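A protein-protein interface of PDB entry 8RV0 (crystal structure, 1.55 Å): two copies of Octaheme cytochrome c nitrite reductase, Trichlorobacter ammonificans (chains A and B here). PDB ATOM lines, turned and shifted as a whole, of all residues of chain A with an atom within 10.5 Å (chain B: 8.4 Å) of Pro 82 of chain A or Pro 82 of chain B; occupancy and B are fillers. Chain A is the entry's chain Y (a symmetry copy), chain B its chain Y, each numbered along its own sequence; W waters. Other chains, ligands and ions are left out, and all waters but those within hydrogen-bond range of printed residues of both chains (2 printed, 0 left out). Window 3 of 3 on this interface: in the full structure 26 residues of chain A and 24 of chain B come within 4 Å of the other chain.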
ATOM      1  N   LYS A  77     -23.183  30.335   4.856  1.00  0.00           N
ATOM      2  CA  LYS A  77     -22.540  29.172   4.225  1.00  0.00           C
ATOM      3  C   LYS A  77     -21.883  29.627   2.915  1.00  0.00           C
ATOM      4  O   LYS A  77     -22.550  29.750   1.901  1.00  0.00           O
ATOM      5  CB  LYS A  77     -23.470  27.996   3.891  1.00  0.00           C
ATOM      6  CG  LYS A  77     -24.234  27.515   5.133  1.00  0.00           C
ATOM      7  CD  LYS A  77     -25.151  26.350   4.827  1.00  0.00           C
ATOM      8  CE  LYS A  77     -25.632  25.794   6.167  1.00  0.00           C
ATOM      9  NZ  LYS A  77     -26.774  24.874   5.962  1.00  0.00           N
ATOM     10  N   GLU A  78     -20.571  29.797   2.952  1.00  0.00           N
ATOM     11  CA  GLU A  78     -19.800  30.125   1.750  1.00  0.00           C
ATOM     12  C   GLU A  78     -19.986  29.018   0.693  1.00  0.00           C
ATOM     13  O   GLU A  78     -19.833  27.824   0.984  1.00  0.00           O
ATOM     14  CB  GLU A  78     -18.347  30.446   2.148  1.00  0.00           C
ATOM     15  CG  GLU A  78     -17.423  30.556   0.965  1.00  0.00           C
ATOM     16  CD  GLU A  78     -17.646  31.697  -0.029  1.00  0.00           C
ATOM     17  OE1 GLU A  78     -17.859  32.892   0.418  1.00  0.00           O
ATOM     18  OE2 GLU A  78     -17.622  31.366  -1.233  1.00  0.00           O
ATOM     19  N   LYS A  79     -20.185  29.411  -0.561  1.00  0.00           N
ATOM     20  CA  LYS A  79     -20.436  28.433  -1.603  1.00  0.00           C
ATOM     21  C   LYS A  79     -19.164  27.724  -2.088  1.00  0.00           C
ATOM     22  O   LYS A  79     -19.224  26.617  -2.607  1.00  0.00           O
ATOM     23  CB  LYS A  79     -21.259  29.068  -2.747  1.00  0.00           C
ATOM     24  CG  LYS A  79     -22.723  29.267  -2.306  1.00  0.00           C
ATOM     25  CD  LYS A  79     -23.463  30.183  -3.225  1.00  0.00           C
ATOM     26  CE  LYS A  79     -23.707  29.463  -4.561  1.00  0.00           C
ATOM     27  NZ  LYS A  79     -24.668  30.335  -5.308  1.00  0.00           N
ATOM     28  N   GLY A  80     -18.045  28.479  -1.984  1.00  0.00           N
ATOM     29  CA  GLY A  80     -16.770  28.155  -2.581  1.00  0.00           C
ATOM     30  C   GLY A  80     -15.919  27.286  -1.663  1.00  0.00           C
ATOM     31  O   GLY A  80     -14.848  27.761  -1.215  1.00  0.00           O
ATOM     32  N   ILE A  81     -16.514  26.206  -1.109  1.00  0.00           N
ATOM     33  CA  ILE A  81     -15.789  25.239  -0.303  1.00  0.00           C
ATOM     34  C   ILE A  81     -15.971  23.844  -0.923  1.00  0.00           C
ATOM     35  O   ILE A  81     -16.887  23.578  -1.715  1.00  0.00           O
ATOM     36  CB  ILE A  81     -16.273  25.252   1.159  1.00  0.00           C
ATOM     37  CG1 ILE A  81     -17.710  24.743   1.175  1.00  0.00           C
ATOM     38  CG2 ILE A  81     -16.062  26.647   1.751  1.00  0.00           C
ATOM     39  CD1 ILE A  81     -18.285  24.520   2.610  1.00  0.00           C
ATOM     40  N   PRO A  82     -15.091  22.875  -0.647  1.00  0.00           N
ATOM     41  CA  PRO A  82     -15.111  21.617  -1.397  1.00  0.00           C
ATOM     42  C   PRO A  82     -16.449  20.895  -1.392  1.00  0.00           C
ATOM     43  O   PRO A  82     -16.900  20.436  -2.449  1.00  0.00           O
ATOM     44  CB  PRO A  82     -14.006  20.767  -0.684  1.00  0.00           C
ATOM     45  CG  PRO A  82     -13.035  21.795  -0.148  1.00  0.00           C
ATOM     46  CD  PRO A  82     -13.914  22.984   0.267  1.00  0.00           C
ATOM     47  N   ALA A  83     -17.122  20.948  -0.223  1.00  0.00           N
ATOM     48  CA  ALA A  83     -18.416  20.281  -0.157  1.00  0.00           C
ATOM     49  C   ALA A  83     -19.593  21.238  -0.427  1.00  0.00           C
ATOM     50  O   ALA A  83     -20.742  20.848  -0.159  1.00  0.00           O
ATOM     51  CB  ALA A  83     -18.575  19.654   1.218  1.00  0.00           C
ATOM     52  N   GLY A  84     -19.363  22.456  -0.941  1.00  0.00           N
ATOM     53  CA  GLY A  84     -20.413  23.444  -1.070  1.00  0.00           C
ATOM     54  C   GLY A  84     -21.020  23.406  -2.464  1.00  0.00           C
ATOM     55  O   GLY A  84     -20.766  22.504  -3.265  1.00  0.00           O
ATOM     56  N   ARG A  85     -21.849  24.419  -2.737  1.00  0.00           N
ATOM     57  CA  ARG A  85     -22.658  24.445  -3.949  1.00  0.00           C
ATOM     58  C   ARG A  85     -21.835  24.894  -5.151  1.00  0.00           C
ATOM     59  O   ARG A  85     -22.234  24.675  -6.286  1.00  0.00           O
ATOM     60  CB  ARG A  85     -23.926  25.325  -3.843  1.00  0.00           C
ATOM     61  CG  ARG A  85     -24.992  24.662  -2.963  1.00  0.00           C
ATOM     62  CD  ARG A  85     -26.343  25.349  -3.243  1.00  0.00           C
ATOM     63  NE  ARG A  85     -26.679  25.135  -4.635  1.00  0.00           N
ATOM     64  CZ  ARG A  85     -26.784  26.066  -5.597  1.00  0.00           C
ATOM     65  NH1 ARG A  85     -26.756  27.361  -5.281  1.00  0.00           N
ATOM     66  NH2 ARG A  85     -27.025  25.642  -6.858  1.00  0.00           N
ATOM     67  N   SER A  86     -20.645  25.451  -4.896  1.00  0.00           N
ATOM     68  CA  SER A  86     -19.812  25.954  -5.996  1.00  0.00           C
ATOM     69  C   SER A  86     -18.311  25.824  -5.693  1.00  0.00           C
ATOM     70  O   SER A  86     -17.580  26.830  -5.387  1.00  0.00           O
ATOM     71  CB  SER A  86     -20.280  27.336  -6.422  1.00  0.00           C
ATOM     72  OG  SER A  86     -19.515  27.885  -7.544  1.00  0.00           O
ATOM     73  N   PRO A  87     -17.807  24.564  -5.670  1.00  0.00           N
ATOM     74  CA  PRO A  87     -16.507  24.265  -5.070  1.00  0.00           C
ATOM     75  C   PRO A  87     -15.337  24.866  -5.814  1.00  0.00           C
ATOM     76  O   PRO A  87     -14.306  25.043  -5.189  1.00  0.00           O
ATOM     77  CB  PRO A  87     -16.397  22.722  -5.251  1.00  0.00           C
ATOM     78  CG  PRO A  87     -17.389  22.351  -6.374  1.00  0.00           C
ATOM     79  CD  PRO A  87     -18.516  23.318  -6.110  1.00  0.00           C
ATOM     80  N   LEU A  88     -15.554  25.209  -7.089  1.00  0.00           N
ATOM     81  CA  LEU A  88     -14.441  25.741  -7.911  1.00  0.00           C
ATOM     82  C   LEU A  88     -14.695  27.214  -8.194  1.00  0.00           C
ATOM     83  O   LEU A  88     -14.128  27.766  -9.133  1.00  0.00           O
ATOM     84  CB  LEU A  88     -14.360  24.948  -9.217  1.00  0.00           C
ATOM     85  CG  LEU A  88     -13.307  23.851  -9.191  1.00  0.00           C
ATOM     86  CD1 LEU A  88     -13.424  22.832 -10.360  1.00  0.00           C
ATOM     87  CD2 LEU A  88     -11.910  24.531  -9.270  1.00  0.00           C
ATOM     88  N   GLN A  89     -15.514  27.873  -7.345  1.00  0.00           N
ATOM     89  CA  GLN A  89     -15.860  29.294  -7.481  1.00  0.00           C
ATOM     90  C   GLN A  89     -14.638  30.206  -7.561  1.00  0.00           C
ATOM     91  O   GLN A  89     -14.639  31.072  -8.445  1.00  0.00           O
ATOM     92  CB  GLN A  89     -16.807  29.742  -6.357  1.00  0.00           C
ATOM     93  CG  GLN A  89     -16.969  31.260  -6.179  1.00  0.00           C
ATOM     94  CD  GLN A  89     -18.075  31.330  -5.169  1.00  0.00           C
ATOM     95  OE1 GLN A  89     -19.248  31.080  -5.508  1.00  0.00           O
ATOM     96  NE2 GLN A  89     -17.686  31.515  -3.908  1.00  0.00           N
ATOM     97  N   ASP A  90     -13.648  30.018  -6.645  1.00  0.00           N
ATOM     98  CA  ASP A  90     -12.538  30.943  -6.632  1.00  0.00           C
ATOM     99  C   ASP A  90     -11.810  30.856  -7.992  1.00  0.00           C
ATOM    100  O   ASP A  90     -11.356  31.881  -8.459  1.00  0.00           O
ATOM    101  CB  ASP A  90     -11.572  30.618  -5.487  1.00  0.00           C
ATOM    102  CG  ASP A  90     -12.104  31.164  -4.158  1.00  0.00           C
ATOM    103  OD1 ASP A  90     -12.222  32.411  -3.949  1.00  0.00           O
ATOM    104  OD2 ASP A  90     -12.439  30.329  -3.332  1.00  0.00           O
ATOM    105  N   GLU A 104     -24.779  31.011   0.699  1.00  0.00           N
ATOM    106  CA  GLU A 104     -26.125  30.576   0.386  1.00  0.00           C
ATOM    107  C   GLU A 104     -27.146  31.541   0.980  1.00  0.00           C
ATOM    108  O   GLU A 104     -26.816  32.263   1.939  1.00  0.00           O
ATOM    109  CB  GLU A 104     -26.345  29.242   1.064  1.00  0.00           C
ATOM    110  CG  GLU A 104     -25.570  28.182   0.295  1.00  0.00           C
ATOM    111  CD  GLU A 104     -25.832  26.744   0.709  1.00  0.00           C
ATOM    112  OE1 GLU A 104     -26.900  26.470   1.358  1.00  0.00           O
ATOM    113  OE2 GLU A 104     -24.965  25.912   0.454  1.00  0.00           O
ATOM    114  N   LYS A 407     -26.253  17.818  -9.990  1.00  0.00           N
ATOM    115  CA  LYS A 407     -24.938  18.093  -9.392  1.00  0.00           C
ATOM    116  C   LYS A 407     -23.794  17.279 -10.020  1.00  0.00           C
ATOM    117  O   LYS A 407     -22.685  17.817 -10.134  1.00  0.00           O
ATOM    118  CB  LYS A 407     -24.940  18.011  -7.872  1.00  0.00           C
ATOM    119  CG  LYS A 407     -25.843  19.138  -7.370  1.00  0.00           C
ATOM    120  CD  LYS A 407     -25.817  19.274  -5.826  1.00  0.00           C
ATOM    121  CE  LYS A 407     -26.645  18.237  -5.193  1.00  0.00           C
ATOM    122  NZ  LYS A 407     -26.430  18.204  -3.731  1.00  0.00           N
ATOM    123  N   ARG A 411     -20.572  19.354 -11.397  1.00  0.00           N
ATOM    124  CA  ARG A 411     -19.196  19.151 -10.924  1.00  0.00           C
ATOM    125  C   ARG A 411     -18.348  18.756 -12.126  1.00  0.00           C
ATOM    126  O   ARG A 411     -17.246  19.285 -12.272  1.00  0.00           O
ATOM    127  CB  ARG A 411     -19.198  17.971  -9.943  1.00  0.00           C
ATOM    128  CG  ARG A 411     -19.821  18.305  -8.576  1.00  0.00           C
ATOM    129  CD  ARG A 411     -19.401  19.483  -7.695  1.00  0.00           C
ATOM    130  NE  ARG A 411     -19.927  20.785  -8.203  1.00  0.00           N
ATOM    131  CZ  ARG A 411     -21.069  21.371  -7.791  1.00  0.00           C
ATOM    132  NH1 ARG A 411     -21.381  22.560  -8.270  1.00  0.00           N
ATOM    133  NH2 ARG A 411     -21.966  20.752  -7.001  1.00  0.00           N
ATOM    134  N   GLU A 414     -17.546  21.890 -14.052  1.00  0.00           N
ATOM    135  CA  GLU A 414     -16.497  22.599 -13.337  1.00  0.00           C
ATOM    136  C   GLU A 414     -15.122  21.964 -13.601  1.00  0.00           C
ATOM    137  O   GLU A 414     -14.123  22.709 -13.743  1.00  0.00           O
ATOM    138  CB  GLU A 414     -16.812  22.625 -11.855  1.00  0.00           C
ATOM    139  CG  GLU A 414     -18.006  23.510 -11.589  1.00  0.00           C
ATOM    140  CD  GLU A 414     -18.669  23.240 -10.254  1.00  0.00           C
ATOM    141  OE1 GLU A 414     -18.112  22.378  -9.499  1.00  0.00           O
ATOM    142  OE2 GLU A 414     -19.618  23.919  -9.948  1.00  0.00           O
ATOM    143  N   GLU B  78      -9.068  10.937   8.906  1.00  0.00           N
ATOM    144  CA  GLU B  78      -7.983  11.641   8.218  1.00  0.00           C
ATOM    145  C   GLU B  78      -8.443  13.064   7.841  1.00  0.00           C
ATOM    146  O   GLU B  78      -9.514  13.255   7.252  1.00  0.00           O
ATOM    147  CB  GLU B  78      -7.460  10.769   7.062  1.00  0.00           C
ATOM    148  CG  GLU B  78      -6.516  11.504   6.149  1.00  0.00           C
ATOM    149  CD  GLU B  78      -5.172  11.967   6.714  1.00  0.00           C
ATOM    150  OE1 GLU B  78      -4.471  11.149   7.430  1.00  0.00           O
ATOM    151  OE2 GLU B  78      -4.859  13.146   6.442  1.00  0.00           O
ATOM    152  N   LYS B  79      -7.580  14.052   8.059  1.00  0.00           N
ATOM    153  CA  LYS B  79      -7.961  15.427   7.793  1.00  0.00           C
ATOM    154  C   LYS B  79      -7.915  15.792   6.304  1.00  0.00           C
ATOM    155  O   LYS B  79      -8.594  16.712   5.865  1.00  0.00           O
ATOM    156  CB  LYS B  79      -7.146  16.390   8.688  1.00  0.00           C
ATOM    157  CG  LYS B  79      -7.648  16.322  10.144  1.00  0.00           C
ATOM    158  CD  LYS B  79      -6.684  16.952  11.096  1.00  0.00           C
ATOM    159  CE  LYS B  79      -6.710  18.476  10.900  1.00  0.00           C
ATOM    160  NZ  LYS B  79      -5.934  19.034  12.052  1.00  0.00           N
ATOM    161  N   GLY B  80      -6.999  15.090   5.598  1.00  0.00           N
ATOM    162  CA  GLY B  80      -6.584  15.396   4.248  1.00  0.00           C
ATOM    163  C   GLY B  80      -7.473  14.718   3.214  1.00  0.00           C
ATOM    164  O   GLY B  80      -6.967  13.842   2.472  1.00  0.00           O
ATOM    165  N   ILE B  81      -8.810  14.836   3.377  1.00  0.00           N
ATOM    166  CA  ILE B  81      -9.766  14.330   2.406  1.00  0.00           C
ATOM    167  C   ILE B  81     -10.669  15.488   1.954  1.00  0.00           C
ATOM    168  O   ILE B  81     -10.793  16.535   2.604  1.00  0.00           O
ATOM    169  CB  ILE B  81     -10.606  13.181   2.994  1.00  0.00           C
ATOM    170  CG1 ILE B  81     -11.478  13.765   4.101  1.00  0.00           C
ATOM    171  CG2 ILE B  81      -9.680  12.040   3.418  1.00  0.00           C
ATOM    172  CD1 ILE B  81     -12.527  12.761   4.675  1.00  0.00           C
ATOM    173  N   PRO B  82     -11.325  15.402   0.790  1.00  0.00           N
ATOM    174  CA  PRO B  82     -12.004  16.573   0.232  1.00  0.00           C
ATOM    175  C   PRO B  82     -13.014  17.227   1.161  1.00  0.00           C
ATOM    176  O   PRO B  82     -13.024  18.458   1.285  1.00  0.00           O
ATOM    177  CB  PRO B  82     -12.701  15.997  -1.047  1.00  0.00           C
ATOM    178  CG  PRO B  82     -11.813  14.847  -1.467  1.00  0.00           C
ATOM    179  CD  PRO B  82     -11.310  14.241  -0.150  1.00  0.00           C
ATOM    180  N   ALA B  83     -13.740  16.369   1.909  1.00  0.00           N
ATOM    181  CA  ALA B  83     -14.720  16.934   2.827  1.00  0.00           C
ATOM    182  C   ALA B  83     -14.170  17.100   4.257  1.00  0.00           C
ATOM    183  O   ALA B  83     -14.974  17.339   5.174  1.00  0.00           O
ATOM    184  CB  ALA B  83     -15.944  16.034   2.854  1.00  0.00           C
ATOM    185  N   GLY B  84     -12.852  16.990   4.485  1.00  0.00           N
ATOM    186  CA  GLY B  84     -12.304  16.986   5.826  1.00  0.00           C
ATOM    187  C   GLY B  84     -11.854  18.382   6.228  1.00  0.00           C
ATOM    188  O   GLY B  84     -12.132  19.380   5.558  1.00  0.00           O
ATOM    189  N   ARG B  85     -11.150  18.433   7.362  1.00  0.00           N
ATOM    190  CA  ARG B  85     -10.797  19.699   7.992  1.00  0.00           C
ATOM    191  C   ARG B  85      -9.597  20.342   7.305  1.00  0.00           C
ATOM    192  O   ARG B  85      -9.356  21.529   7.472  1.00  0.00           O
ATOM    193  CB  ARG B  85     -10.519  19.594   9.511  1.00  0.00           C
ATOM    194  CG  ARG B  85     -11.815  19.386  10.302  1.00  0.00           C
ATOM    195  CD  ARG B  85     -11.536  19.719  11.780  1.00  0.00           C
ATOM    196  NE  ARG B  85     -11.149  21.110  11.866  1.00  0.00           N
ATOM    197  CZ  ARG B  85      -9.955  21.599  12.241  1.00  0.00           C
ATOM    198  NH1 ARG B  85      -9.034  20.789  12.766  1.00  0.00           N
ATOM    199  NH2 ARG B  85      -9.772  22.937  12.169  1.00  0.00           N
ATOM    200  N   SER B  86      -8.893  19.569   6.469  1.00  0.00           N
ATOM    201  CA  SER B  86      -7.694  20.097   5.806  1.00  0.00           C
ATOM    202  C   SER B  86      -7.482  19.478   4.415  1.00  0.00           C
ATOM    203  O   SER B  86      -6.576  18.603   4.183  1.00  0.00           O
ATOM    204  CB  SER B  86      -6.501  20.033   6.745  1.00  0.00           C
ATOM    205  OG  SER B  86      -5.274  20.580   6.159  1.00  0.00           O
ATOM    206  N   PRO B  87      -8.370  19.833   3.453  1.00  0.00           N
ATOM    207  CA  PRO B  87      -8.501  19.079   2.208  1.00  0.00           C
ATOM    208  C   PRO B  87      -7.288  19.164   1.310  1.00  0.00           C
ATOM    209  O   PRO B  87      -7.123  18.267   0.503  1.00  0.00           O
ATOM    210  CB  PRO B  87      -9.646  19.834   1.472  1.00  0.00           C
ATOM    211  CG  PRO B  87      -9.720  21.234   2.118  1.00  0.00           C
ATOM    212  CD  PRO B  87      -9.402  20.916   3.557  1.00  0.00           C
ATOM    213  N   LEU B  88      -6.462  20.195   1.522  1.00  0.00           N
ATOM    214  CA  LEU B  88      -5.285  20.393   0.642  1.00  0.00           C
ATOM    215  C   LEU B  88      -4.020  20.109   1.435  1.00  0.00           C
ATOM    216  O   LEU B  88      -2.940  20.549   1.050  1.00  0.00           O
ATOM    217  CB  LEU B  88      -5.286  21.833   0.123  1.00  0.00           C
ATOM    218  CG  LEU B  88      -5.872  21.970  -1.273  1.00  0.00           C
ATOM    219  CD1 LEU B  88      -6.184  23.436  -1.689  1.00  0.00           C
ATOM    220  CD2 LEU B  88      -4.843  21.382  -2.282  1.00  0.00           C
ATOM    221  N   GLN B  89      -4.140  19.323   2.529  1.00  0.00           N
ATOM    222  CA  GLN B  89      -3.016  18.958   3.399  1.00  0.00           C
ATOM    223  C   GLN B  89      -1.850  18.324   2.644  1.00  0.00           C
ATOM    224  O   GLN B  89      -0.715  18.743   2.906  1.00  0.00           O
ATOM    225  CB  GLN B  89      -3.481  18.052   4.551  1.00  0.00           C
ATOM    226  CG  GLN B  89      -2.370  17.325   5.325  1.00  0.00           C
ATOM    227  CD  GLN B  89      -3.141  16.716   6.458  1.00  0.00           C
ATOM    228  OE1 GLN B  89      -3.546  17.432   7.394  1.00  0.00           O
ATOM    229  NE2 GLN B  89      -3.472  15.435   6.300  1.00  0.00           N
ATOM    230  N   ASP B  90      -2.137  17.333   1.756  1.00  0.00           N
ATOM    231  CA  ASP B  90      -1.039  16.642   1.117  1.00  0.00           C
ATOM    232  C   ASP B  90      -0.233  17.666   0.286  1.00  0.00           C
ATOM    233  O   ASP B  90       0.974  17.533   0.238  1.00  0.00           O
ATOM    234  CB  ASP B  90      -1.557  15.514   0.217  1.00  0.00           C
ATOM    235  CG  ASP B  90      -1.911  14.277   1.049  1.00  0.00           C
ATOM    236  OD1 ASP B  90      -1.024  13.620   1.677  1.00  0.00           O
ATOM    237  OD2 ASP B  90      -3.096  13.989   1.100  1.00  0.00           O
ATOM    238  N   LYS B 407     -14.453  28.643   8.026  1.00  0.00           N
ATOM    239  CA  LYS B 407     -14.106  27.652   6.996  1.00  0.00           C
ATOM    240  C   LYS B 407     -14.118  28.219   5.567  1.00  0.00           C
ATOM    241  O   LYS B 407     -13.280  27.798   4.761  1.00  0.00           O
ATOM    242  CB  LYS B 407     -14.904  26.360   7.112  1.00  0.00           C
ATOM    243  CG  LYS B 407     -14.499  25.709   8.436  1.00  0.00           C
ATOM    244  CD  LYS B 407     -15.121  24.301   8.616  1.00  0.00           C
ATOM    245  CE  LYS B 407     -16.532  24.396   9.017  1.00  0.00           C
ATOM    246  NZ  LYS B 407     -17.194  23.075   8.950  1.00  0.00           N
ATOM    247  N   GLY B 408     -15.027  29.118   5.233  1.00  0.00           N
ATOM    248  CA  GLY B 408     -15.008  29.694   3.910  1.00  0.00           C
ATOM    249  C   GLY B 408     -13.655  30.395   3.654  1.00  0.00           C
ATOM    250  O   GLY B 408     -13.091  30.276   2.540  1.00  0.00           O
ATOM    251  N   MET B 410     -10.863  29.704   5.341  1.00  0.00           N
ATOM    252  CA  MET B 410      -9.787  28.708   5.371  1.00  0.00           C
ATOM    253  C   MET B 410      -9.629  28.067   3.987  1.00  0.00           C
ATOM    254  O   MET B 410      -8.510  27.838   3.513  1.00  0.00           O
ATOM    255  CB  MET B 410     -10.148  27.632   6.406  1.00  0.00           C
ATOM    256  CG  MET B 410      -9.997  28.180   7.820  1.00  0.00           C
ATOM    257  SD  MET B 410     -10.646  26.950   9.055  1.00  0.00           S
ATOM    258  CE  MET B 410      -9.283  25.782   8.864  1.00  0.00           C
ATOM    259  N   ARG B 411     -10.756  27.699   3.329  1.00  0.00           N
ATOM    260  CA  ARG B 411     -10.723  26.996   2.041  1.00  0.00           C
ATOM    261  C   ARG B 411     -10.209  27.974   0.992  1.00  0.00           C
ATOM    262  O   ARG B 411      -9.363  27.586   0.187  1.00  0.00           O
ATOM    263  CB  ARG B 411     -12.163  26.621   1.664  1.00  0.00           C
ATOM    264  CG  ARG B 411     -12.738  25.462   2.498  1.00  0.00           C
ATOM    265  CD  ARG B 411     -12.064  24.100   2.673  1.00  0.00           C
ATOM    266  NE  ARG B 411     -10.915  24.157   3.624  1.00  0.00           N
ATOM    267  CZ  ARG B 411     -10.985  23.870   4.940  1.00  0.00           C
ATOM    268  NH1 ARG B 411      -9.876  23.888   5.654  1.00  0.00           N
ATOM    269  NH2 ARG B 411     -12.150  23.677   5.586  1.00  0.00           N
ATOM    270  N   LYS B 412     -10.544  29.260   1.190  1.00  0.00           N
ATOM    271  CA  LYS B 412     -10.111  30.244   0.193  1.00  0.00           C
ATOM    272  C   LYS B 412      -8.605  30.452   0.401  1.00  0.00           C
ATOM    273  O   LYS B 412      -7.878  30.619  -0.581  1.00  0.00           O
ATOM    274  CB  LYS B 412     -10.928  31.530   0.340  1.00  0.00           C
ATOM    275  CG  LYS B 412     -10.733  32.575  -0.754  1.00  0.00           C
ATOM    276  CD  LYS B 412     -11.591  33.889  -0.366  1.00  0.00           C
ATOM    277  CE  LYS B 412     -13.079  33.626  -0.283  1.00  0.00           C
ATOM    278  NZ  LYS B 412     -13.546  32.971  -1.553  1.00  0.00           N
ATOM    279  N   GLU B 414      -6.463  28.160   1.331  1.00  0.00           N
ATOM    280  CA  GLU B 414      -5.899  26.962   0.729  1.00  0.00           C
ATOM    281  C   GLU B 414      -5.867  27.078  -0.804  1.00  0.00           C
ATOM    282  O   GLU B 414      -4.878  26.626  -1.429  1.00  0.00           O
ATOM    283  CB  GLU B 414      -6.686  25.744   1.170  1.00  0.00           C
ATOM    284  CG  GLU B 414      -6.458  25.478   2.639  1.00  0.00           C
ATOM    285  CD  GLU B 414      -7.525  24.604   3.264  1.00  0.00           C
ATOM    286  OE1 GLU B 414      -8.423  24.144   2.483  1.00  0.00           O
ATOM    287  OE2 GLU B 414      -7.409  24.319   4.430  1.00  0.00           O
HETATM  288  O   HOH W   1     -14.314  30.256  -0.160  1.00  0.00           O
HETATM  289  O   HOH W   2     -16.291  33.603  -2.247  1.00  0.00           O
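Printed residues of chain A that touch a printed residue of chain B: Glu 78, Ile 81, Pro 82 and Asp 90.
Hydrophobic or aromatic side chains of chain A within 4 Å of the printed part of chain B: Ile 81 and Pro 82.
Among the printed residues, Asp or Glu carboxylates within 4 Å of a Lys or Arg side-chain nitrogen of the other chain: Asp 90 of chain A with Lys 412 of chain B.
The side-chain amino group (NZ) of Lys 412 of chain B is in salt-bridge range of the side-chain carboxylate (OD1) of Asp 90 of chain A, at 2.8 Å.
O of Arg 85 of chain B sits at hydrogen-bond distance from NH1 of Arg 411 of chain B.
The guanidinium group of Arg 411 of chain B is in salt-bridge range of the side-chain carboxylate of Glu 414 of chain B, at 2.7 Å.
OE2 of Glu 78 of chain A lies within hydrogen-bond range of N of Gly 80 of chain A (3.0 Å).
The side-chain amide nitrogen (NE2) of Gln 89 of chain A sits at hydrogen-bond distance from the side-chain carboxylate (OE2) of Glu 78 of chain A.
Of the printed residues of chain B, Glu 78 of chain A touches Gly 408.
Pro 82 of chain A touches just these residues of chain B: Pro 82 and Arg 411.
Of chain A, only Pro 82 (3.2 Å) comes within 4 Å of Pro 82 of chain B.
No residue of chain A comes within 4 Å of Ala 83 of chain B.
Gly 84 of chain B touches none of the printed residues of chain A.
No residue of chain A comes within 4 Å of Pro 87 of chain B.
Of the printed residues of chain A, Gly 408 of chain B touches Glu 78 and Ile 81.
Of the printed residues of chain A, Arg 411 of chain B touches Ile 81 and Pro 82.
The nearest residue of chain A that does not touch Pro 82 of chain B is Ala 83 of chain A (5.0 Å).
Ile 81 of chain A touches Arg 411 of chain B, but with the chains exchanged Arg 411 of chain A does not touch Ile 81 of chain B (13.6 Å).
Pro 82 of chain A touches its own counterpart, Pro 82 of chain B.
Pro 82 of chain A touches Arg 411 of chain B, but with the chains exchanged Arg 411 of chain A does not touch Pro 82 of chain B (10.1 Å).
Of the 6 pairs that touch across the chains among the printed residues, 1 has its exchanged pair printed and touching as well.
Water W1 lies within hydrogen-bond range of the backbone carbonyl oxygen (O) of Gly 80 of chain A (2.8 Å), the backbone carbonyl oxygen (O) of Gly 408 of chain B (3.0 Å) and the side-chain amino group (NZ) of Lys 412 of chain B (3.1 Å).
Water W2 lies within hydrogen-bond range of OE2 of Glu 78 of chain A, NZ of Lys 412 of chain B and NE2 of Gln 89 of chain A.
Among the printed residues, pairs that only touch across the chains: Pro 82 of chain A with Pro 82 of chain B, Pro 82 of chain A with Arg 411 of chain B, Ile 81 of chain A with Arg 411 of chain B, Glu 78 of chain A with Gly 408 of chain B and Ile 81 of chain A with Gly 408 of chain B.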
